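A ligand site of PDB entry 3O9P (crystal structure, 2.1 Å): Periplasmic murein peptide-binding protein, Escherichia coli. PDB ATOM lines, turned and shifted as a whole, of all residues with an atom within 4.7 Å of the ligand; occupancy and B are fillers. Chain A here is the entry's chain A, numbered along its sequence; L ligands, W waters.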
ATOM      1  N   LYS A  24     -28.321  14.421   8.064  1.00  0.00           N
ATOM      2  CA  LYS A  24     -27.040  14.641   7.419  1.00  0.00           C
ATOM      3  C   LYS A  24     -27.039  14.787   5.913  1.00  0.00           C
ATOM      4  O   LYS A  24     -26.158  15.416   5.347  1.00  0.00           O
ATOM      5  CB  LYS A  24     -26.050  13.527   7.779  1.00  0.00           C
ATOM      6  CG  LYS A  24     -25.664  13.482   9.241  1.00  0.00           C
ATOM      7  CD  LYS A  24     -24.211  12.971   9.474  1.00  0.00           C
ATOM      8  CE  LYS A  24     -23.925  11.467   9.328  1.00  0.00           C
ATOM      9  NZ  LYS A  24     -25.009  10.562   8.997  1.00  0.00           N
ATOM     10  N   VAL A  36     -32.282   3.065   0.671  1.00  0.00           N
ATOM     11  CA  VAL A  36     -31.200   2.223   1.058  1.00  0.00           C
ATOM     12  C   VAL A  36     -30.439   2.645   2.327  1.00  0.00           C
ATOM     13  O   VAL A  36     -29.879   1.779   2.962  1.00  0.00           O
ATOM     14  CB  VAL A  36     -30.237   2.025  -0.085  1.00  0.00           C
ATOM     15  CG1 VAL A  36     -29.333   3.239  -0.248  1.00  0.00           C
ATOM     16  CG2 VAL A  36     -29.394   0.723   0.149  1.00  0.00           C
ATOM     17  N   GLY A  37     -30.493   3.947   2.695  1.00  0.00           N
ATOM     18  CA  GLY A  37     -29.846   4.464   3.868  1.00  0.00           C
ATOM     19  C   GLY A  37     -30.623   5.450   4.723  1.00  0.00           C
ATOM     20  O   GLY A  37     -31.729   5.875   4.391  1.00  0.00           O
ATOM     21  N   LEU A  38     -29.987   5.851   5.804  1.00  0.00           N
ATOM     22  CA  LEU A  38     -30.670   6.605   6.844  1.00  0.00           C
ATOM     23  C   LEU A  38     -31.182   7.978   6.471  1.00  0.00           C
ATOM     24  O   LEU A  38     -32.129   8.430   7.112  1.00  0.00           O
ATOM     25  CB  LEU A  38     -29.853   6.665   8.159  1.00  0.00           C
ATOM     26  CG  LEU A  38     -29.603   5.299   8.849  1.00  0.00           C
ATOM     27  CD1 LEU A  38     -28.932   5.467  10.217  1.00  0.00           C
ATOM     28  CD2 LEU A  38     -30.983   4.587   9.021  1.00  0.00           C
ATOM     29  N   PRO A  39     -30.579   8.668   5.468  1.00  0.00           N
ATOM     30  CA  PRO A  39     -31.193   9.948   5.156  1.00  0.00           C
ATOM     31  C   PRO A  39     -32.683   9.777   4.738  1.00  0.00           C
ATOM     32  O   PRO A  39     -33.529  10.480   5.302  1.00  0.00           O
ATOM     33  CB  PRO A  39     -30.336  10.482   4.017  1.00  0.00           C
ATOM     34  CG  PRO A  39     -28.978   9.885   4.273  1.00  0.00           C
ATOM     35  CD  PRO A  39     -29.243   8.540   4.870  1.00  0.00           C
ATOM     36  N   ILE A  41     -34.542   6.905   5.151  1.00  0.00           N
ATOM     37  CA  ILE A  41     -35.216   5.992   6.045  1.00  0.00           C
ATOM     38  C   ILE A  41     -35.796   6.827   7.197  1.00  0.00           C
ATOM     39  O   ILE A  41     -36.915   6.598   7.560  1.00  0.00           O
ATOM     40  CB  ILE A  41     -34.326   4.848   6.578  1.00  0.00           C
ATOM     41  CG1 ILE A  41     -34.023   3.866   5.471  1.00  0.00           C
ATOM     42  CG2 ILE A  41     -34.974   4.112   7.730  1.00  0.00           C
ATOM     43  CD1 ILE A  41     -32.795   2.971   5.720  1.00  0.00           C
ATOM     44  N   PHE A 113     -33.159  -3.477  -1.572  1.00  0.00           N
ATOM     45  CA  PHE A 113     -33.407  -4.341  -0.404  1.00  0.00           C
ATOM     46  C   PHE A 113     -34.151  -5.730  -0.703  1.00  0.00           C
ATOM     47  O   PHE A 113     -34.643  -6.421   0.194  1.00  0.00           O
ATOM     48  CB  PHE A 113     -34.116  -3.484   0.658  1.00  0.00           C
ATOM     49  CG  PHE A 113     -33.221  -3.098   1.820  1.00  0.00           C
ATOM     50  CD1 PHE A 113     -32.192  -2.203   1.669  1.00  0.00           C
ATOM     51  CD2 PHE A 113     -33.431  -3.615   3.069  1.00  0.00           C
ATOM     52  CE1 PHE A 113     -31.372  -1.868   2.771  1.00  0.00           C
ATOM     53  CE2 PHE A 113     -32.637  -3.279   4.156  1.00  0.00           C
ATOM     54  CZ  PHE A 113     -31.598  -2.417   3.991  1.00  0.00           C
ATOM     55  N   PHE A 166     -38.053  -0.851   7.245  1.00  0.00           N
ATOM     56  CA  PHE A 166     -38.668  -0.052   6.221  1.00  0.00           C
ATOM     57  C   PHE A 166     -38.993  -0.813   4.951  1.00  0.00           C
ATOM     58  O   PHE A 166     -39.962  -0.453   4.282  1.00  0.00           O
ATOM     59  CB  PHE A 166     -37.808   1.184   5.849  1.00  0.00           C
ATOM     60  CG  PHE A 166     -36.609   0.865   5.106  1.00  0.00           C
ATOM     61  CD1 PHE A 166     -36.602   0.888   3.706  1.00  0.00           C
ATOM     62  CD2 PHE A 166     -35.430   0.494   5.767  1.00  0.00           C
ATOM     63  CE1 PHE A 166     -35.492   0.491   2.987  1.00  0.00           C
ATOM     64  CE2 PHE A 166     -34.298   0.061   5.047  1.00  0.00           C
ATOM     65  CZ  PHE A 166     -34.325   0.093   3.673  1.00  0.00           C
ATOM     66  N   GLU A 248     -28.153  15.318  13.657  1.00  0.00           N
ATOM     67  CA  GLU A 248     -27.504  14.036  13.462  1.00  0.00           C
ATOM     68  C   GLU A 248     -26.019  14.251  13.394  1.00  0.00           C
ATOM     69  O   GLU A 248     -25.495  14.785  12.405  1.00  0.00           O
ATOM     70  CB  GLU A 248     -28.038  13.404  12.178  1.00  0.00           C
ATOM     71  CG  GLU A 248     -27.725  11.882  11.962  1.00  0.00           C
ATOM     72  CD  GLU A 248     -28.228  11.426  10.566  1.00  0.00           C
ATOM     73  OE1 GLU A 248     -27.555  10.540   9.975  1.00  0.00           O
ATOM     74  OE2 GLU A 248     -29.242  12.032  10.010  1.00  0.00           O
ATOM     75  N   SER A 249     -25.325  13.768  14.429  1.00  0.00           N
ATOM     76  CA  SER A 249     -23.903  13.950  14.611  1.00  0.00           C
ATOM     77  C   SER A 249     -23.595  15.443  14.854  1.00  0.00           C
ATOM     78  O   SER A 249     -24.504  16.233  15.062  1.00  0.00           O
ATOM     79  CB  SER A 249     -23.080  13.443  13.438  1.00  0.00           C
ATOM     80  OG  SER A 249     -21.683  13.311  13.803  1.00  0.00           O
ATOM     81  N   GLN A 271     -24.246   2.621  19.188  1.00  0.00           N
ATOM     82  CA  GLN A 271     -25.268   2.350  18.176  1.00  0.00           C
ATOM     83  C   GLN A 271     -24.928   1.052  17.476  1.00  0.00           C
ATOM     84  O   GLN A 271     -23.767   0.690  17.346  1.00  0.00           O
ATOM     85  CB  GLN A 271     -25.284   3.477  17.138  1.00  0.00           C
ATOM     86  CG  GLN A 271     -26.285   3.344  16.028  1.00  0.00           C
ATOM     87  CD  GLN A 271     -26.539   4.617  15.241  1.00  0.00           C
ATOM     88  OE1 GLN A 271     -25.947   5.713  15.541  1.00  0.00           O
ATOM     89  NE2 GLN A 271     -27.406   4.509  14.188  1.00  0.00           N
ATOM     90  N   HIS A 373     -15.868  12.038   7.258  1.00  0.00           N
ATOM     91  CA  HIS A 373     -15.317  11.103   6.291  1.00  0.00           C
ATOM     92  C   HIS A 373     -14.093  11.596   5.577  1.00  0.00           C
ATOM     93  O   HIS A 373     -13.197  10.804   5.191  1.00  0.00           O
ATOM     94  CB  HIS A 373     -16.338  10.600   5.253  1.00  0.00           C
ATOM     95  CG  HIS A 373     -17.586  10.080   5.898  1.00  0.00           C
ATOM     96  ND1 HIS A 373     -18.811  10.068   5.252  1.00  0.00           N
ATOM     97  CD2 HIS A 373     -17.823   9.680   7.171  1.00  0.00           C
ATOM     98  CE1 HIS A 373     -19.736   9.660   6.101  1.00  0.00           C
ATOM     99  NE2 HIS A 373     -19.175   9.432   7.256  1.00  0.00           N
ATOM    100  N   TRP A 399     -24.323  11.790  -1.016  1.00  0.00           N
ATOM    101  CA  TRP A 399     -24.925  10.549  -0.684  1.00  0.00           C
ATOM    102  C   TRP A 399     -25.657   9.970  -1.901  1.00  0.00           C
ATOM    103  O   TRP A 399     -25.298   8.914  -2.395  1.00  0.00           O
ATOM    104  CB  TRP A 399     -25.777  10.678   0.611  1.00  0.00           C
ATOM    105  CG  TRP A 399     -26.820   9.637   0.777  1.00  0.00           C
ATOM    106  CD1 TRP A 399     -28.148   9.757   0.514  1.00  0.00           C
ATOM    107  CD2 TRP A 399     -26.593   8.285   1.178  1.00  0.00           C
ATOM    108  NE1 TRP A 399     -28.792   8.558   0.794  1.00  0.00           N
ATOM    109  CE2 TRP A 399     -27.836   7.641   1.169  1.00  0.00           C
ATOM    110  CE3 TRP A 399     -25.454   7.561   1.552  1.00  0.00           C
ATOM    111  CZ2 TRP A 399     -27.973   6.266   1.517  1.00  0.00           C
ATOM    112  CZ3 TRP A 399     -25.578   6.215   1.906  1.00  0.00           C
ATOM    113  CH2 TRP A 399     -26.837   5.582   1.865  1.00  0.00           C
ATOM    114  N   TYR A 402     -23.174   9.049  -4.585  1.00  0.00           N
ATOM    115  CA  TYR A 402     -22.297   7.979  -4.022  1.00  0.00           C
ATOM    116  C   TYR A 402     -22.959   6.595  -4.091  1.00  0.00           C
ATOM    117  O   TYR A 402     -22.302   5.594  -4.487  1.00  0.00           O
ATOM    118  CB  TYR A 402     -21.933   8.333  -2.604  1.00  0.00           C
ATOM    119  CG  TYR A 402     -21.592   7.214  -1.624  1.00  0.00           C
ATOM    120  CD1 TYR A 402     -20.291   6.700  -1.509  1.00  0.00           C
ATOM    121  CD2 TYR A 402     -22.545   6.718  -0.773  1.00  0.00           C
ATOM    122  CE1 TYR A 402     -19.975   5.670  -0.561  1.00  0.00           C
ATOM    123  CE2 TYR A 402     -22.247   5.698   0.154  1.00  0.00           C
ATOM    124  CZ  TYR A 402     -20.961   5.182   0.276  1.00  0.00           C
ATOM    125  OH  TYR A 402     -20.771   4.195   1.241  1.00  0.00           O
ATOM    126  N   ARG A 406     -20.677   3.827  -6.298  1.00  0.00           N
ATOM    127  CA  ARG A 406     -20.001   2.751  -5.564  1.00  0.00           C
ATOM    128  C   ARG A 406     -20.276   1.302  -6.092  1.00  0.00           C
ATOM    129  O   ARG A 406     -19.495   0.400  -5.826  1.00  0.00           O
ATOM    130  CB  ARG A 406     -20.360   2.837  -4.082  1.00  0.00           C
ATOM    131  CG  ARG A 406     -21.786   2.401  -3.710  1.00  0.00           C
ATOM    132  CD  ARG A 406     -22.051   2.470  -2.184  1.00  0.00           C
ATOM    133  NE  ARG A 406     -23.472   2.225  -1.945  1.00  0.00           N
ATOM    134  CZ  ARG A 406     -24.052   2.159  -0.750  1.00  0.00           C
ATOM    135  NH1 ARG A 406     -23.340   2.352   0.363  1.00  0.00           N
ATOM    136  NH2 ARG A 406     -25.362   1.868  -0.653  1.00  0.00           N
ATOM    137  N   ARG A 415     -15.515   3.998   1.099  1.00  0.00           N
ATOM    138  CA  ARG A 415     -16.011   4.213   2.445  1.00  0.00           C
ATOM    139  C   ARG A 415     -17.502   3.891   2.557  1.00  0.00           C
ATOM    140  O   ARG A 415     -18.277   4.248   1.674  1.00  0.00           O
ATOM    141  CB  ARG A 415     -15.820   5.675   2.869  1.00  0.00           C
ATOM    142  CG  ARG A 415     -16.301   5.966   4.332  1.00  0.00           C
ATOM    143  CD  ARG A 415     -17.794   6.442   4.466  1.00  0.00           C
ATOM    144  NE  ARG A 415     -18.415   6.132   5.750  1.00  0.00           N
ATOM    145  CZ  ARG A 415     -19.723   6.326   6.004  1.00  0.00           C
ATOM    146  NH1 ARG A 415     -20.488   6.852   5.046  1.00  0.00           N
ATOM    147  NH2 ARG A 415     -20.275   6.028   7.179  1.00  0.00           N
ATOM    148  N   SER A 417     -20.807   2.673   5.685  1.00  0.00           N
ATOM    149  CA  SER A 417     -21.265   2.052   6.887  1.00  0.00           C
ATOM    150  C   SER A 417     -22.404   1.063   6.676  1.00  0.00           C
ATOM    151  O   SER A 417     -23.090   1.074   5.600  1.00  0.00           O
ATOM    152  CB  SER A 417     -21.685   3.069   7.919  1.00  0.00           C
ATOM    153  OG  SER A 417     -22.875   3.755   7.592  1.00  0.00           O
ATOM    154  N   TRP A 418     -22.661   0.259   7.729  1.00  0.00           N
ATOM    155  CA  TRP A 418     -23.890  -0.557   7.818  1.00  0.00           C
ATOM    156  C   TRP A 418     -24.395  -0.437   9.230  1.00  0.00           C
ATOM    157  O   TRP A 418     -23.629  -0.672  10.151  1.00  0.00           O
ATOM    158  CB  TRP A 418     -23.556  -2.056   7.599  1.00  0.00           C
ATOM    159  CG  TRP A 418     -24.772  -2.895   7.368  1.00  0.00           C
ATOM    160  CD1 TRP A 418     -25.354  -3.724   8.260  1.00  0.00           C
ATOM    161  CD2 TRP A 418     -25.608  -2.913   6.201  1.00  0.00           C
ATOM    162  NE1 TRP A 418     -26.444  -4.319   7.720  1.00  0.00           N
ATOM    163  CE2 TRP A 418     -26.615  -3.856   6.440  1.00  0.00           C
ATOM    164  CE3 TRP A 418     -25.536  -2.279   4.948  1.00  0.00           C
ATOM    165  CZ2 TRP A 418     -27.634  -4.136   5.489  1.00  0.00           C
ATOM    166  CZ3 TRP A 418     -26.547  -2.567   3.955  1.00  0.00           C
ATOM    167  CH2 TRP A 418     -27.587  -3.485   4.255  1.00  0.00           C
ATOM    168  N   VAL A 419     -25.646  -0.010   9.376  1.00  0.00           N
ATOM    169  CA  VAL A 419     -26.365  -0.048  10.583  1.00  0.00           C
ATOM    170  C   VAL A 419     -27.402  -1.233  10.421  1.00  0.00           C
ATOM    171  O   VAL A 419     -28.141  -1.351   9.419  1.00  0.00           O
ATOM    172  CB  VAL A 419     -27.100   1.275  10.811  1.00  0.00           C
ATOM    173  CG1 VAL A 419     -26.105   2.502  10.922  1.00  0.00           C
ATOM    174  CG2 VAL A 419     -27.853   1.577   9.636  1.00  0.00           C
ATOM    175  N   ASP A 421     -30.381  -3.770  10.433  1.00  0.00           N
ATOM    176  CA  ASP A 421     -31.781  -3.683  10.132  1.00  0.00           C
ATOM    177  C   ASP A 421     -32.570  -4.350  11.220  1.00  0.00           C
ATOM    178  O   ASP A 421     -33.753  -4.232  11.247  1.00  0.00           O
ATOM    179  CB  ASP A 421     -32.066  -4.288   8.780  1.00  0.00           C
ATOM    180  CG  ASP A 421     -31.336  -3.552   7.694  1.00  0.00           C
ATOM    181  OD1 ASP A 421     -31.385  -2.324   7.651  1.00  0.00           O
ATOM    182  OD2 ASP A 421     -30.659  -4.220   6.892  1.00  0.00           O
ATOM    183  N   TYR A 487     -20.125   2.573  15.854  1.00  0.00           N
ATOM    184  CA  TYR A 487     -20.761   3.855  16.010  1.00  0.00           C
ATOM    185  C   TYR A 487     -21.260   4.197  17.365  1.00  0.00           C
ATOM    186  O   TYR A 487     -21.633   3.324  18.172  1.00  0.00           O
ATOM    187  CB  TYR A 487     -21.945   3.953  15.070  1.00  0.00           C
ATOM    188  CG  TYR A 487     -21.641   4.450  13.690  1.00  0.00           C
ATOM    189  CD1 TYR A 487     -21.327   3.584  12.674  1.00  0.00           C
ATOM    190  CD2 TYR A 487     -21.685   5.780  13.398  1.00  0.00           C
ATOM    191  CE1 TYR A 487     -21.007   4.042  11.373  1.00  0.00           C
ATOM    192  CE2 TYR A 487     -21.413   6.245  12.080  1.00  0.00           C
ATOM    193  CZ  TYR A 487     -21.096   5.397  11.087  1.00  0.00           C
ATOM    194  OH  TYR A 487     -20.824   5.864   9.811  1.00  0.00           O
ATOM    195  N   THR A 488     -21.305   5.522  17.585  1.00  0.00           N
ATOM    196  CA  THR A 488     -22.174   6.108  18.599  1.00  0.00           C
ATOM    197  C   THR A 488     -23.189   6.999  17.902  1.00  0.00           C
ATOM    198  O   THR A 488     -22.960   7.511  16.789  1.00  0.00           O
ATOM    199  CB  THR A 488     -21.365   6.954  19.675  1.00  0.00           C
ATOM    200  OG1 THR A 488     -20.568   7.913  18.983  1.00  0.00           O
ATOM    201  CG2 THR A 488     -20.509   6.043  20.598  1.00  0.00           C
ATOM    202  N   ASN A 489     -24.334   7.127  18.552  1.00  0.00           N
ATOM    203  CA  ASN A 489     -25.429   7.865  18.045  1.00  0.00           C
ATOM    204  C   ASN A 489     -25.289   9.303  18.518  1.00  0.00           C
ATOM    205  O   ASN A 489     -26.022   9.754  19.420  1.00  0.00           O
ATOM    206  CB  ASN A 489     -26.727   7.276  18.568  1.00  0.00           C
ATOM    207  CG  ASN A 489     -27.988   7.910  17.945  1.00  0.00           C
ATOM    208  OD1 ASN A 489     -27.931   8.561  16.907  1.00  0.00           O
ATOM    209  ND2 ASN A 489     -29.142   7.634  18.561  1.00  0.00           N
ATOM    210  N   GLY A 490     -24.332   9.997  17.923  1.00  0.00           N
ATOM    211  CA  GLY A 490     -23.959  11.360  18.342  1.00  0.00           C
ATOM    212  C   GLY A 490     -25.025  12.321  17.976  1.00  0.00           C
ATOM    213  O   GLY A 490     -25.339  12.475  16.809  1.00  0.00           O
HETATM  214  C1  LIG L   1     -30.057   0.799   6.369  1.00  0.00           C
HETATM  215  N1  LIG L   1     -29.025  -1.346   6.791  1.00  0.00           N
HETATM  216  O1  LIG L   1     -26.915   0.299   6.710  1.00  0.00           O
HETATM  217  C2  LIG L   1     -29.007  -0.255   5.856  1.00  0.00           C
HETATM  218  N2  LIG L   1     -27.301   1.059   4.672  1.00  0.00           N
HETATM  219  O2  LIG L   1     -26.495   1.409   2.112  1.00  0.00           O
HETATM  220  C3  LIG L   1     -27.641   0.387   5.773  1.00  0.00           C
HETATM  221  N3  LIG L   1     -25.395   5.024   7.741  1.00  0.00           N
HETATM  222  O3  LIG L   1     -24.503   1.969   2.705  1.00  0.00           O
HETATM  223  C4  LIG L   1     -25.998   1.690   4.495  1.00  0.00           C
HETATM  224  N4  LIG L   1     -25.201   8.007  14.423  1.00  0.00           N
HETATM  225  O4  LIG L   1     -27.110   5.600   6.417  1.00  0.00           O
HETATM  226  C5  LIG L   1     -25.612   1.663   3.058  1.00  0.00           C
HETATM  227  O5  LIG L   1     -23.802   8.295   7.931  1.00  0.00           O
HETATM  228  C6  LIG L   1     -25.971   3.139   4.961  1.00  0.00           C
HETATM  229  O6  LIG L   1     -23.152   6.435   7.103  1.00  0.00           O
HETATM  230  C7  LIG L   1     -26.433   3.275   6.413  1.00  0.00           C
HETATM  231  O7  LIG L   1     -23.559   9.823  11.912  1.00  0.00           O
HETATM  232  C8  LIG L   1     -26.338   4.738   6.852  1.00  0.00           C
HETATM  233  O8  LIG L   1     -22.976   9.053  13.930  1.00  0.00           O
HETATM  234  C9  LIG L   1     -25.233   6.312   8.358  1.00  0.00           C
HETATM  235  C10 LIG L   1     -23.992   7.001   7.779  1.00  0.00           C
HETATM  236  C11 LIG L   1     -25.098   6.047   9.837  1.00  0.00           C
HETATM  237  C12 LIG L   1     -24.798   7.297  10.656  1.00  0.00           C
HETATM  238  C13 LIG L   1     -24.953   7.090  12.147  1.00  0.00           C
HETATM  239  C14 LIG L   1     -23.780   9.102  12.994  1.00  0.00           C
HETATM  240  C15 LIG L   1     -25.049   8.343  13.023  1.00  0.00           C
HETATM  241  O   HOH W   1     -25.772  10.196   6.198  1.00  0.00           O
HETATM  242  O   HOH W   2     -21.033  10.257  11.476  1.00  0.00           O
HETATM  243  O   HOH W   3     -26.420  10.215  15.395  1.00  0.00           O
HETATM  244  O   HOH W   4     -22.622   9.560   5.873  1.00  0.00           O
HETATM  245  O   HOH W   5     -30.633   0.794   9.698  1.00  0.00           O
HETATM  246  O   HOH W   6     -25.809   7.677   5.091  1.00  0.00           O
HETATM  247  O   HOH W   7     -22.430   3.766   3.463  1.00  0.00           O
HETATM  248  O   HOH W   8     -22.775  -0.656   3.516  1.00  0.00           O
HETATM  249  O   HOH W   9     -28.097   7.407  13.705  1.00  0.00           O
HETATM  250  O   HOH W  10     -23.320   6.250   4.461  1.00  0.00           O
HETATM  251  O   HOH W  11     -21.725  11.052  15.075  1.00  0.00           O
HETATM  252  O   HOH W  12     -21.172   8.322   9.254  1.00  0.00           O
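NH1 of Arg 406 lies within salt-bridge range of O3 of the ligand (2.6 Å). A nitrogen (N4) of the ligand lies within hydrogen-bond range of the side-chain amide oxygen of Gln 271, at 2.7 Å. OD1 of Asp 421 is in salt-bridge range of N1 of the ligand. A nitrogen (N1) of the ligand lies within hydrogen-bond range of the backbone carbonyl oxygen (O) of Val 419 (2.8 Å). N2 of the ligand is in hydrogen-bond range of O of Val 36 (3.2 Å). O4 of the ligand sits at hydrogen-bond distance from N of Leu 38 (3.0 Å). NH2 of Arg 415 lies within salt-bridge range of O6 of the ligand (2.9 Å). The side-chain hydroxyl (OG) of Ser 417 is in hydrogen-bond range of an oxygen (O6) of the ligand, 2.7 Å away. A nitrogen (N4) of the ligand is in hydrogen-bond range of the backbone carbonyl oxygen of Thr 488, at 3.3 Å. O1 of the ligand sits at hydrogen-bond distance from N of Val 419, 3.0 Å away. NZ of Lys 24 is in salt-bridge range of O5 of the ligand (2.8 Å).
OH of Tyr 402 is in hydrogen-bond range of NH1 of Arg 406 (3.3 Å). The side-chain carboxylate (OE1) of Glu 248 is in salt-bridge range of the side-chain amino group (NZ) of Lys 24 (2.7 Å). O of Arg 415 is in hydrogen-bond range of OH of Tyr 402 (2.5 Å). NH2 of Arg 415 lies within hydrogen-bond range of OH of Tyr 487, at 2.7 Å. The side-chain hydroxyl (OG) of Ser 417 lies close to the guanidinium group (NH2) of Arg 415 (3.5 Å). The backbone NH (N) of Ser 249 is in hydrogen-bond range of the backbone carbonyl oxygen (O) of Gly 490 (2.7 Å). N of Gln 271 sits at hydrogen-bond distance from O of Tyr 487 (2.9 Å).
C of Gly 37 touches O4 of the ligand (3.9 Å). Pro 39 touches the ligand. Ile 41 touches the ligand (CD1 to C1, 3.6 Å). Phe 113 touches the ligand (CZ to C2, 3.9 Å). Ser 249 touches the ligand. Trp 418 touches the ligand. Tyr 487 touches the ligand. Asn 489 touches the ligand. Hydrophobic or aromatic side chains that line the ligand: Val 36, Leu 38, Pro 39, Ile 41, Phe 113, Trp 418, Val 419 and Tyr 487. 18 residues have an atom within 4 Å of the ligand: Lys 24, Val 36, Gly 37, Leu 38, Pro 39, Ile 41, Phe 113, Ser 249, Gln 271, Arg 406, Arg 415, Ser 417, Trp 418, Val 419, Asp 421, Tyr 487, Thr 488 and Asn 489. The nearest printed residue that does not touch the ligand is Trp 399 (4.04 Å).
Water W10 bridges O6 of the ligand (2.7 Å) and NH1 of Arg 415 (3.0 Å). Water W3 lies within hydrogen-bond range of OD1 of Asn 489 (2.7 Å), N4 of the ligand (2.7 Å) and O of Gly 490 (2.9 Å). Water W7 lies within hydrogen-bond range of OH of Tyr 402, O3 of the ligand and N of Ser 417. Water W12 lies within hydrogen-bond range of the side-chain hydroxyl of Tyr 487, an oxygen (O5) of the ligand, a ring nitrogen (NE2) of His 373 and the guanidinium group of Arg 415. Water W9 lies within hydrogen-bond range of the side-chain amide nitrogen of Gln 271 (3.0 Å), a nitrogen (N4) of the ligand (3.0 Å) and the side-chain amide oxygen of Asn 489 (3.4 Å). Water W1 bridges NZ of Lys 24 (2.9 Å) and O5 of the ligand (3.2 Å).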
